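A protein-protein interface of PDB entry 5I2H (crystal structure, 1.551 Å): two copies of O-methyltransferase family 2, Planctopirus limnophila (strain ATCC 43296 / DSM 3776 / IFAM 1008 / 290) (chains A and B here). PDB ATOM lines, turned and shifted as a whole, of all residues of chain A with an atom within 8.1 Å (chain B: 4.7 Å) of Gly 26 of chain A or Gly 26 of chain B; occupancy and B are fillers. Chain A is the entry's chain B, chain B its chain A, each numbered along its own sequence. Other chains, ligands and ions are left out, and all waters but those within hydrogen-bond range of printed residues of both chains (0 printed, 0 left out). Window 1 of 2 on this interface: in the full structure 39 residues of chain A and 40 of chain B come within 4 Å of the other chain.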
ATOM      1  N   ILE A  20       8.502  -0.593 -32.371  1.00  0.00           N
ATOM      2  CA  ILE A  20       8.272   0.856 -32.341  1.00  0.00           C
ATOM      3  C   ILE A  20       7.641   1.280 -31.007  1.00  0.00           C
ATOM      4  O   ILE A  20       8.005   2.313 -30.431  1.00  0.00           O
ATOM      5  CB  ILE A  20       7.399   1.283 -33.545  1.00  0.00           C
ATOM      6  CG1 ILE A  20       8.178   1.149 -34.847  1.00  0.00           C
ATOM      7  CG2 ILE A  20       6.877   2.718 -33.345  1.00  0.00           C
ATOM      8  CD1 ILE A  20       7.312   1.108 -36.087  1.00  0.00           C
ATOM      9  N   PHE A  21       6.658   0.520 -30.520  1.00  0.00           N
ATOM     10  CA  PHE A  21       6.073   0.832 -29.210  1.00  0.00           C
ATOM     11  C   PHE A  21       7.134   0.785 -28.120  1.00  0.00           C
ATOM     12  O   PHE A  21       7.164   1.635 -27.227  1.00  0.00           O
ATOM     13  CB  PHE A  21       4.934  -0.146 -28.871  1.00  0.00           C
ATOM     14  CG  PHE A  21       3.671   0.110 -29.629  1.00  0.00           C
ATOM     15  CD1 PHE A  21       2.877   1.218 -29.328  1.00  0.00           C
ATOM     16  CD2 PHE A  21       3.238  -0.761 -30.603  1.00  0.00           C
ATOM     17  CE1 PHE A  21       1.670   1.438 -30.016  1.00  0.00           C
ATOM     18  CE2 PHE A  21       2.042  -0.517 -31.316  1.00  0.00           C
ATOM     19  CZ  PHE A  21       1.276   0.570 -31.028  1.00  0.00           C
ATOM     20  N   ASP A  22       8.017  -0.217 -28.169  1.00  0.00           N
ATOM     21  CA  ASP A  22       9.041  -0.335 -27.138  1.00  0.00           C
ATOM     22  C   ASP A  22       9.983   0.859 -27.170  1.00  0.00           C
ATOM     23  O   ASP A  22      10.302   1.433 -26.116  1.00  0.00           O
ATOM     24  CB  ASP A  22       9.803  -1.645 -27.318  1.00  0.00           C
ATOM     25  CG  ASP A  22       8.922  -2.868 -27.094  1.00  0.00           C
ATOM     26  OD1 ASP A  22       7.825  -2.728 -26.491  1.00  0.00           O
ATOM     27  OD2 ASP A  22       9.321  -3.975 -27.525  1.00  0.00           O
ATOM     28  N   LEU A  23      10.383   1.292 -28.370  1.00  0.00           N
ATOM     29  CA  LEU A  23      11.280   2.447 -28.473  1.00  0.00           C
ATOM     30  C   LEU A  23      10.588   3.685 -27.950  1.00  0.00           C
ATOM     31  O   LEU A  23      11.205   4.528 -27.277  1.00  0.00           O
ATOM     32  CB  LEU A  23      11.718   2.687 -29.920  1.00  0.00           C
ATOM     33  CG  LEU A  23      12.765   1.730 -30.468  1.00  0.00           C
ATOM     34  CD1 LEU A  23      12.807   1.816 -31.953  1.00  0.00           C
ATOM     35  CD2 LEU A  23      14.136   2.147 -29.870  1.00  0.00           C
ATOM     36  N   PHE A  24       9.293   3.801 -28.254  1.00  0.00           N
ATOM     37  CA  PHE A  24       8.522   4.968 -27.877  1.00  0.00           C
ATOM     38  C   PHE A  24       8.432   5.141 -26.365  1.00  0.00           C
ATOM     39  O   PHE A  24       8.213   6.266 -25.916  1.00  0.00           O
ATOM     40  CB  PHE A  24       7.125   4.849 -28.515  1.00  0.00           C
ATOM     41  CG  PHE A  24       6.225   6.005 -28.227  1.00  0.00           C
ATOM     42  CD1 PHE A  24       6.516   7.275 -28.732  1.00  0.00           C
ATOM     43  CD2 PHE A  24       5.081   5.819 -27.472  1.00  0.00           C
ATOM     44  CE1 PHE A  24       5.669   8.369 -28.472  1.00  0.00           C
ATOM     45  CE2 PHE A  24       4.196   6.898 -27.208  1.00  0.00           C
ATOM     46  CZ  PHE A  24       4.501   8.178 -27.703  1.00  0.00           C
ATOM     47  N   ARG A  25       8.608   4.065 -25.564  1.00  0.00           N
ATOM     48  CA  ARG A  25       8.512   4.216 -24.112  1.00  0.00           C
ATOM     49  C   ARG A  25       9.805   4.661 -23.466  1.00  0.00           C
ATOM     50  O   ARG A  25       9.855   4.718 -22.228  1.00  0.00           O
ATOM     51  CB  ARG A  25       8.139   2.920 -23.399  1.00  0.00           C
ATOM     52  CG  ARG A  25       7.215   2.027 -24.072  1.00  0.00           C
ATOM     53  CD  ARG A  25       5.843   2.558 -23.960  1.00  0.00           C
ATOM     54  NE  ARG A  25       4.876   1.636 -24.556  1.00  0.00           N
ATOM     55  CZ  ARG A  25       3.676   2.021 -24.962  1.00  0.00           C
ATOM     56  NH1 ARG A  25       3.323   3.312 -24.836  1.00  0.00           N
ATOM     57  NH2 ARG A  25       2.841   1.151 -25.512  1.00  0.00           N
ATOM     58  N   GLY A  26      10.838   4.987 -24.254  1.00  0.00           N
ATOM     59  CA  GLY A  26      12.145   5.260 -23.677  1.00  0.00           C
ATOM     60  C   GLY A  26      12.182   6.412 -22.688  1.00  0.00           C
ATOM     61  O   GLY A  26      12.984   6.391 -21.755  1.00  0.00           O
ATOM     62  N   ASN A  27      11.327   7.430 -22.870  1.00  0.00           N
ATOM     63  CA  ASN A  27      11.354   8.549 -21.924  1.00  0.00           C
ATOM     64  C   ASN A  27      11.093   8.090 -20.491  1.00  0.00           C
ATOM     65  O   ASN A  27      11.627   8.694 -19.543  1.00  0.00           O
ATOM     66  CB  ASN A  27      10.306   9.594 -22.282  1.00  0.00           C
ATOM     67  CG  ASN A  27       8.889   9.054 -22.167  1.00  0.00           C
ATOM     68  OD1 ASN A  27       8.521   8.174 -22.931  1.00  0.00           O
ATOM     69  ND2 ASN A  27       8.091   9.572 -21.193  1.00  0.00           N
ATOM     70  N   PHE A  28      10.276   7.042 -20.305  1.00  0.00           N
ATOM     71  CA  PHE A  28      10.007   6.586 -18.946  1.00  0.00           C
ATOM     72  C   PHE A  28      11.224   5.948 -18.298  1.00  0.00           C
ATOM     73  O   PHE A  28      11.312   5.954 -17.068  1.00  0.00           O
ATOM     74  CB  PHE A  28       8.796   5.645 -18.938  1.00  0.00           C
ATOM     75  CG  PHE A  28       7.517   6.396 -19.213  1.00  0.00           C
ATOM     76  CD1 PHE A  28       7.014   7.273 -18.245  1.00  0.00           C
ATOM     77  CD2 PHE A  28       6.892   6.331 -20.470  1.00  0.00           C
ATOM     78  CE1 PHE A  28       5.883   8.035 -18.502  1.00  0.00           C
ATOM     79  CE2 PHE A  28       5.736   7.083 -20.738  1.00  0.00           C
ATOM     80  CZ  PHE A  28       5.230   7.943 -19.756  1.00  0.00           C
ATOM     81  N   ALA A  29      12.178   5.438 -19.085  1.00  0.00           N
ATOM     82  CA  ALA A  29      13.419   4.953 -18.491  1.00  0.00           C
ATOM     83  C   ALA A  29      14.244   6.116 -17.937  1.00  0.00           C
ATOM     84  O   ALA A  29      14.679   6.096 -16.778  1.00  0.00           O
ATOM     85  CB  ALA A  29      14.233   4.139 -19.511  1.00  0.00           C
ATOM     86  N   THR A  30      14.421   7.163 -18.750  1.00  0.00           N
ATOM     87  CA  THR A  30      15.120   8.363 -18.304  1.00  0.00           C
ATOM     88  C   THR A  30      14.449   8.961 -17.073  1.00  0.00           C
ATOM     89  O   THR A  30      15.117   9.313 -16.090  1.00  0.00           O
ATOM     90  CB  THR A  30      15.121   9.378 -19.441  1.00  0.00           C
ATOM     91  OG1 THR A  30      15.639   8.751 -20.613  1.00  0.00           O
ATOM     92  CG2 THR A  30      15.982  10.606 -19.074  1.00  0.00           C
ATOM     93  N   GLU A  31      13.126   9.150 -17.146  1.00  0.00           N
ATOM     94  CA  GLU A  31      12.412   9.799 -16.046  1.00  0.00           C
ATOM     95  C   GLU A  31      12.464   8.967 -14.771  1.00  0.00           C
ATOM     96  O   GLU A  31      12.620   9.518 -13.674  1.00  0.00           O
ATOM     97  CB  GLU A  31      10.959  10.080 -16.461  1.00  0.00           C
ATOM     98  CG  GLU A  31      10.920  11.141 -17.587  1.00  0.00           C
ATOM     99  CD  GLU A  31       9.640  11.103 -18.422  1.00  0.00           C
ATOM    100  OE1 GLU A  31       8.679  10.418 -18.016  1.00  0.00           O
ATOM    101  OE2 GLU A  31       9.579  11.766 -19.492  1.00  0.00           O
ATOM    102  N   LEU A  32      12.300   7.641 -14.873  1.00  0.00           N
ATOM    103  CA  LEU A  32      12.345   6.844 -13.648  1.00  0.00           C
ATOM    104  C   LEU A  32      13.747   6.881 -13.022  1.00  0.00           C
ATOM    105  O   LEU A  32      13.887   6.977 -11.795  1.00  0.00           O
ATOM    106  CB  LEU A  32      11.915   5.394 -13.917  1.00  0.00           C
ATOM    107  CG  LEU A  32      11.877   4.534 -12.641  1.00  0.00           C
ATOM    108  CD1 LEU A  32      10.834   5.093 -11.670  1.00  0.00           C
ATOM    109  CD2 LEU A  32      11.566   3.095 -12.990  1.00  0.00           C
ATOM    110  N   LEU A  33      14.802   6.834 -13.853  1.00  0.00           N
ATOM    111  CA  LEU A  33      16.164   6.942 -13.311  1.00  0.00           C
ATOM    112  C   LEU A  33      16.373   8.281 -12.612  1.00  0.00           C
ATOM    113  O   LEU A  33      16.848   8.326 -11.475  1.00  0.00           O
ATOM    114  CB  LEU A  33      17.208   6.770 -14.418  1.00  0.00           C
ATOM    115  CG  LEU A  33      17.389   5.305 -14.879  1.00  0.00           C
ATOM    116  CD1 LEU A  33      18.158   5.345 -16.188  1.00  0.00           C
ATOM    117  CD2 LEU A  33      18.169   4.511 -13.792  1.00  0.00           C
ATOM    118  N   MET A  77      15.128  -2.880 -14.983  1.00  0.00           N
ATOM    119  CA  MET A  77      16.398  -2.281 -15.395  1.00  0.00           C
ATOM    120  C   MET A  77      17.610  -2.913 -14.691  1.00  0.00           C
ATOM    121  O   MET A  77      18.725  -2.408 -14.813  1.00  0.00           O
ATOM    122  CB  MET A  77      16.386  -0.774 -15.122  1.00  0.00           C
ATOM    123  CG  MET A  77      15.487   0.000 -16.035  1.00  0.00           C
ATOM    124  SD  MET A  77      15.715   1.910 -15.630  1.00  0.00           S
ATOM    125  CE  MET A  77      13.858   2.317 -15.682  1.00  0.00           C
ATOM    126  N   LEU A 316       8.027  -0.309 -18.506  1.00  0.00           N
ATOM    127  CA  LEU A 316       8.018   1.092 -18.921  1.00  0.00           C
ATOM    128  C   LEU A 316       6.631   1.496 -19.389  1.00  0.00           C
ATOM    129  O   LEU A 316       6.169   2.607 -19.099  1.00  0.00           O
ATOM    130  CB  LEU A 316       9.056   1.332 -20.021  1.00  0.00           C
ATOM    131  CG  LEU A 316      10.464   1.025 -19.546  1.00  0.00           C
ATOM    132  CD1 LEU A 316      11.404   1.345 -20.763  1.00  0.00           C
ATOM    133  CD2 LEU A 316      10.953   1.910 -18.371  1.00  0.00           C
ATOM    134  N   TYR A 317       5.950   0.603 -20.104  1.00  0.00           N
ATOM    135  CA  TYR A 317       4.558   0.879 -20.456  1.00  0.00           C
ATOM    136  C   TYR A 317       3.703   1.075 -19.200  1.00  0.00           C
ATOM    137  O   TYR A 317       2.841   1.977 -19.144  1.00  0.00           O
ATOM    138  CB  TYR A 317       4.019  -0.265 -21.315  1.00  0.00           C
ATOM    139  CG  TYR A 317       2.617  -0.081 -21.805  1.00  0.00           C
ATOM    140  CD1 TYR A 317       2.078   1.192 -22.068  1.00  0.00           C
ATOM    141  CD2 TYR A 317       1.848  -1.181 -22.082  1.00  0.00           C
ATOM    142  CE1 TYR A 317       0.771   1.329 -22.563  1.00  0.00           C
ATOM    143  CE2 TYR A 317       0.552  -1.050 -22.550  1.00  0.00           C
ATOM    144  CZ  TYR A 317       0.027   0.186 -22.796  1.00  0.00           C
ATOM    145  OH  TYR A 317      -1.262   0.227 -23.294  1.00  0.00           O
ATOM    146  N   ASP B  22      22.972   3.839 -21.350  1.00  0.00           N
ATOM    147  CA  ASP B  22      22.141   3.547 -22.507  1.00  0.00           C
ATOM    148  C   ASP B  22      20.677   3.695 -22.154  1.00  0.00           C
ATOM    149  O   ASP B  22      19.903   4.285 -22.929  1.00  0.00           O
ATOM    150  CB  ASP B  22      22.448   2.140 -23.029  1.00  0.00           C
ATOM    151  CG  ASP B  22      23.860   2.013 -23.584  1.00  0.00           C
ATOM    152  OD1 ASP B  22      24.495   3.042 -23.871  1.00  0.00           O
ATOM    153  OD2 ASP B  22      24.360   0.874 -23.738  1.00  0.00           O
ATOM    154  N   LEU B  23      20.279   3.193 -20.986  1.00  0.00           N
ATOM    155  CA  LEU B  23      18.876   3.341 -20.569  1.00  0.00           C
ATOM    156  C   LEU B  23      18.533   4.805 -20.404  1.00  0.00           C
ATOM    157  O   LEU B  23      17.427   5.240 -20.744  1.00  0.00           O
ATOM    158  CB  LEU B  23      18.615   2.625 -19.239  1.00  0.00           C
ATOM    159  CG  LEU B  23      18.498   1.112 -19.252  1.00  0.00           C
ATOM    160  CD1 LEU B  23      18.682   0.559 -17.844  1.00  0.00           C
ATOM    161  CD2 LEU B  23      17.117   0.747 -19.801  1.00  0.00           C
ATOM    162  N   PHE B  24      19.475   5.571 -19.838  1.00  0.00           N
ATOM    163  CA  PHE B  24      19.249   6.977 -19.555  1.00  0.00           C
ATOM    164  C   PHE B  24      18.954   7.799 -20.811  1.00  0.00           C
ATOM    165  O   PHE B  24      18.306   8.855 -20.707  1.00  0.00           O
ATOM    166  CB  PHE B  24      20.478   7.522 -18.805  1.00  0.00           C
ATOM    167  CG  PHE B  24      20.380   8.973 -18.435  1.00  0.00           C
ATOM    168  CD1 PHE B  24      19.456   9.398 -17.504  1.00  0.00           C
ATOM    169  CD2 PHE B  24      21.269   9.887 -18.967  1.00  0.00           C
ATOM    170  CE1 PHE B  24      19.368  10.730 -17.136  1.00  0.00           C
ATOM    171  CE2 PHE B  24      21.204  11.239 -18.605  1.00  0.00           C
ATOM    172  CZ  PHE B  24      20.240  11.653 -17.673  1.00  0.00           C
ATOM    173  N   ARG B  25      19.415   7.355 -21.999  1.00  0.00           N
ATOM    174  CA  ARG B  25      19.144   8.116 -23.226  1.00  0.00           C
ATOM    175  C   ARG B  25      17.767   7.858 -23.810  1.00  0.00           C
ATOM    176  O   ARG B  25      17.497   8.340 -24.920  1.00  0.00           O
ATOM    177  CB  ARG B  25      20.117   7.788 -24.345  1.00  0.00           C
ATOM    178  CG  ARG B  25      21.472   7.511 -23.932  1.00  0.00           C
ATOM    179  CD  ARG B  25      22.197   8.745 -23.685  1.00  0.00           C
ATOM    180  NE  ARG B  25      23.592   8.453 -23.380  1.00  0.00           N
ATOM    181  CZ  ARG B  25      24.333   9.288 -22.678  1.00  0.00           C
ATOM    182  NH1 ARG B  25      25.594   9.008 -22.417  1.00  0.00           N
ATOM    183  NH2 ARG B  25      23.769  10.418 -22.217  1.00  0.00           N
ATOM    184  N   GLY B  26      16.918   7.066 -23.139  1.00  0.00           N
ATOM    185  CA  GLY B  26      15.675   6.629 -23.757  1.00  0.00           C
ATOM    186  C   GLY B  26      14.768   7.758 -24.194  1.00  0.00           C
ATOM    187  O   GLY B  26      14.036   7.610 -25.176  1.00  0.00           O
ATOM    188  N   ASN B  27      14.754   8.873 -23.456  1.00  0.00           N
ATOM    189  CA  ASN B  27      13.864   9.974 -23.847  1.00  0.00           C
ATOM    190  C   ASN B  27      14.116  10.435 -25.277  1.00  0.00           C
ATOM    191  O   ASN B  27      13.182  10.905 -25.939  1.00  0.00           O
ATOM    192  CB  ASN B  27      14.023  11.195 -22.929  1.00  0.00           C
ATOM    193  CG  ASN B  27      15.428  11.799 -23.032  1.00  0.00           C
ATOM    194  OD1 ASN B  27      16.409  11.153 -22.644  1.00  0.00           O
ATOM    195  ND2 ASN B  27      15.534  13.009 -23.588  1.00  0.00           N
ATOM    196  N   PHE B  28      15.370  10.364 -25.750  1.00  0.00           N
ATOM    197  CA  PHE B  28      15.631  10.848 -27.098  1.00  0.00           C
ATOM    198  C   PHE B  28      15.032   9.945 -28.153  1.00  0.00           C
ATOM    199  O   PHE B  28      14.776  10.423 -29.267  1.00  0.00           O
ATOM    200  CB  PHE B  28      17.130  11.059 -27.319  1.00  0.00           C
ATOM    201  CG  PHE B  28      17.635  12.236 -26.558  1.00  0.00           C
ATOM    202  CD1 PHE B  28      17.306  13.516 -26.980  1.00  0.00           C
ATOM    203  CD2 PHE B  28      18.367  12.061 -25.372  1.00  0.00           C
ATOM    204  CE1 PHE B  28      17.745  14.631 -26.264  1.00  0.00           C
ATOM    205  CE2 PHE B  28      18.807  13.163 -24.640  1.00  0.00           C
ATOM    206  CZ  PHE B  28      18.480  14.462 -25.086  1.00  0.00           C
ATOM    207  N   ALA B  29      14.801   8.662 -27.844  1.00  0.00           N
ATOM    208  CA  ALA B  29      14.040   7.810 -28.758  1.00  0.00           C
ATOM    209  C   ALA B  29      12.593   8.291 -28.870  1.00  0.00           C
ATOM    210  O   ALA B  29      12.082   8.521 -29.976  1.00  0.00           O
ATOM    211  CB  ALA B  29      14.093   6.353 -28.282  1.00  0.00           C
ATOM    212  N   THR B  30      11.938   8.506 -27.725  1.00  0.00           N
ATOM    213  CA  THR B  30      10.563   9.010 -27.736  1.00  0.00           C
ATOM    214  C   THR B  30      10.476  10.338 -28.477  1.00  0.00           C
ATOM    215  O   THR B  30       9.607  10.541 -29.330  1.00  0.00           O
ATOM    216  CB  THR B  30      10.087   9.204 -26.298  1.00  0.00           C
ATOM    217  OG1 THR B  30      10.304   7.995 -25.585  1.00  0.00           O
ATOM    218  CG2 THR B  30       8.606   9.627 -26.248  1.00  0.00           C
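N of Asn 27 of chain B is in hydrogen-bond range of O of Gly 26 of chain A, at 3.5 Å. The backbone carbonyl oxygen of Phe 24 of chain B sits at hydrogen-bond distance from the side-chain hydroxyl of Thr 30 of chain A (2.7 Å). OG1 of Thr 30 of chain B sits at hydrogen-bond distance from N of Gly 26 of chain A, 3.3 Å away. The side-chain hydroxyl (OG1) of Thr 30 of chain A is in hydrogen-bond range of the backbone NH (N) of Asn 27 of chain B, 3.0 Å away. The side-chain hydroxyl (OG1) of Thr 30 of chain B lies within hydrogen-bond range of the backbone carbonyl oxygen (O) of Phe 24 of chain A (2.7 Å). N of Asn 27 of chain A lies within hydrogen-bond range of OG1 of Thr 30 of chain B (3.0 Å). The backbone NH (N) of Gly 26 of chain B is in hydrogen-bond range of the side-chain hydroxyl (OG1) of Thr 30 of chain A, at 3.3 Å.
The side-chain amide nitrogen (ND2) of Asn 27 of chain A is in hydrogen-bond range of the side-chain carboxylate (OE2) of Glu 31 of chain A (3.1 Å).
Leu 23 of chain A touches Ala 29 of chain B. Leu 23 of chain A touches Thr 30 of chain B (O to OG1, 3.96 Å). Arg 25 of chain A touches Thr 30 of chain B (C to OG1, 3.98 Å). Gly 26 of chain A touches Gly 26 of chain B. O of Gly 26 of chain B touches N of Asn 27 of chain A, at 3.6 Å. Ala 29 of chain A touches Leu 23 of chain B. Thr 30 of chain A touches Leu 23 of chain B. Thr 30 of chain A touches Arg 25 of chain B. Leu 33 of chain A touches Phe 24 of chain B (CD1 to N, 3.9 Å). CG of Met 77 of chain A touches CD1 of Leu 23 of chain B (3.7 Å).
Gly 26 of chain A touches three residues of chain B. Printed residues of chain A within 4 Å of Gly 26 of chain B: Gly 26 (3.3 Å), Asn 27 (3.6 Å) and Thr 30 (3.3 Å). Printed residues of chain B within 4 Å of Thr 30 of chain A: Leu 23 (3.9 Å), Phe 24 (2.7 Å), Arg 25 (3.9 Å), Gly 26 (3.3 Å) and Asn 27 (3.0 Å). Printed residues of chain A within 4 Å of Arg 25 of chain B: Thr 30. Of the printed residues of chain B, Leu 23 of chain A touches Ala 29 and Thr 30. Glu 31 of chain A touches none of the printed residues of chain B. The nearest printed residue of chain B that does not touch Gly 26 of chain A is Leu 23 of chain B (4.7 Å). The nearest residue of chain A that does not touch Gly 26 of chain B is Leu 23 of chain A (4.7 Å). The nearest printed residue of chain B that does not touch Phe 24 of chain A is Ala 29 of chain B (5.3 Å).
Of the 9 printed residues of chain B, 7 touch a printed residue of chain A. Printed residues of chain B that touch a printed residue of chain A: Leu 23, Phe 24, Arg 25, Gly 26, Asn 27, Ala 29 and Thr 30. Hydrophobic or aromatic side chains of chain B within 4 Å of the printed part of chain A: Leu 23, Phe 24 and Ala 29. Along chain B the printed residues that touch a printed residue of chain A span positions 23 to 30. Of the 17 printed residues of chain A, 9 touch a printed residue of chain B. Among the printed residues, no Asp or Glu carboxylate lies within 4 Å of a Lys or Arg side-chain nitrogen of the other chain.
Leu 23 of chain A touches Ala 29 of chain B, and with the chains exchanged Ala 29 of chain A touches Leu 23 of chain B. Leu 23 of chain A touches Thr 30 of chain B, and with the chains exchanged Thr 30 of chain A touches Leu 23 of chain B. Phe 24 of chain A touches Thr 30 of chain B, and with the chains exchanged Thr 30 of chain A touches Phe 24 of chain B. Asn 27 of chain A touches Thr 30 of chain B, and with the chains exchanged Thr 30 of chain A touches Asn 27 of chain B. 9 positions are printed for both chains.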
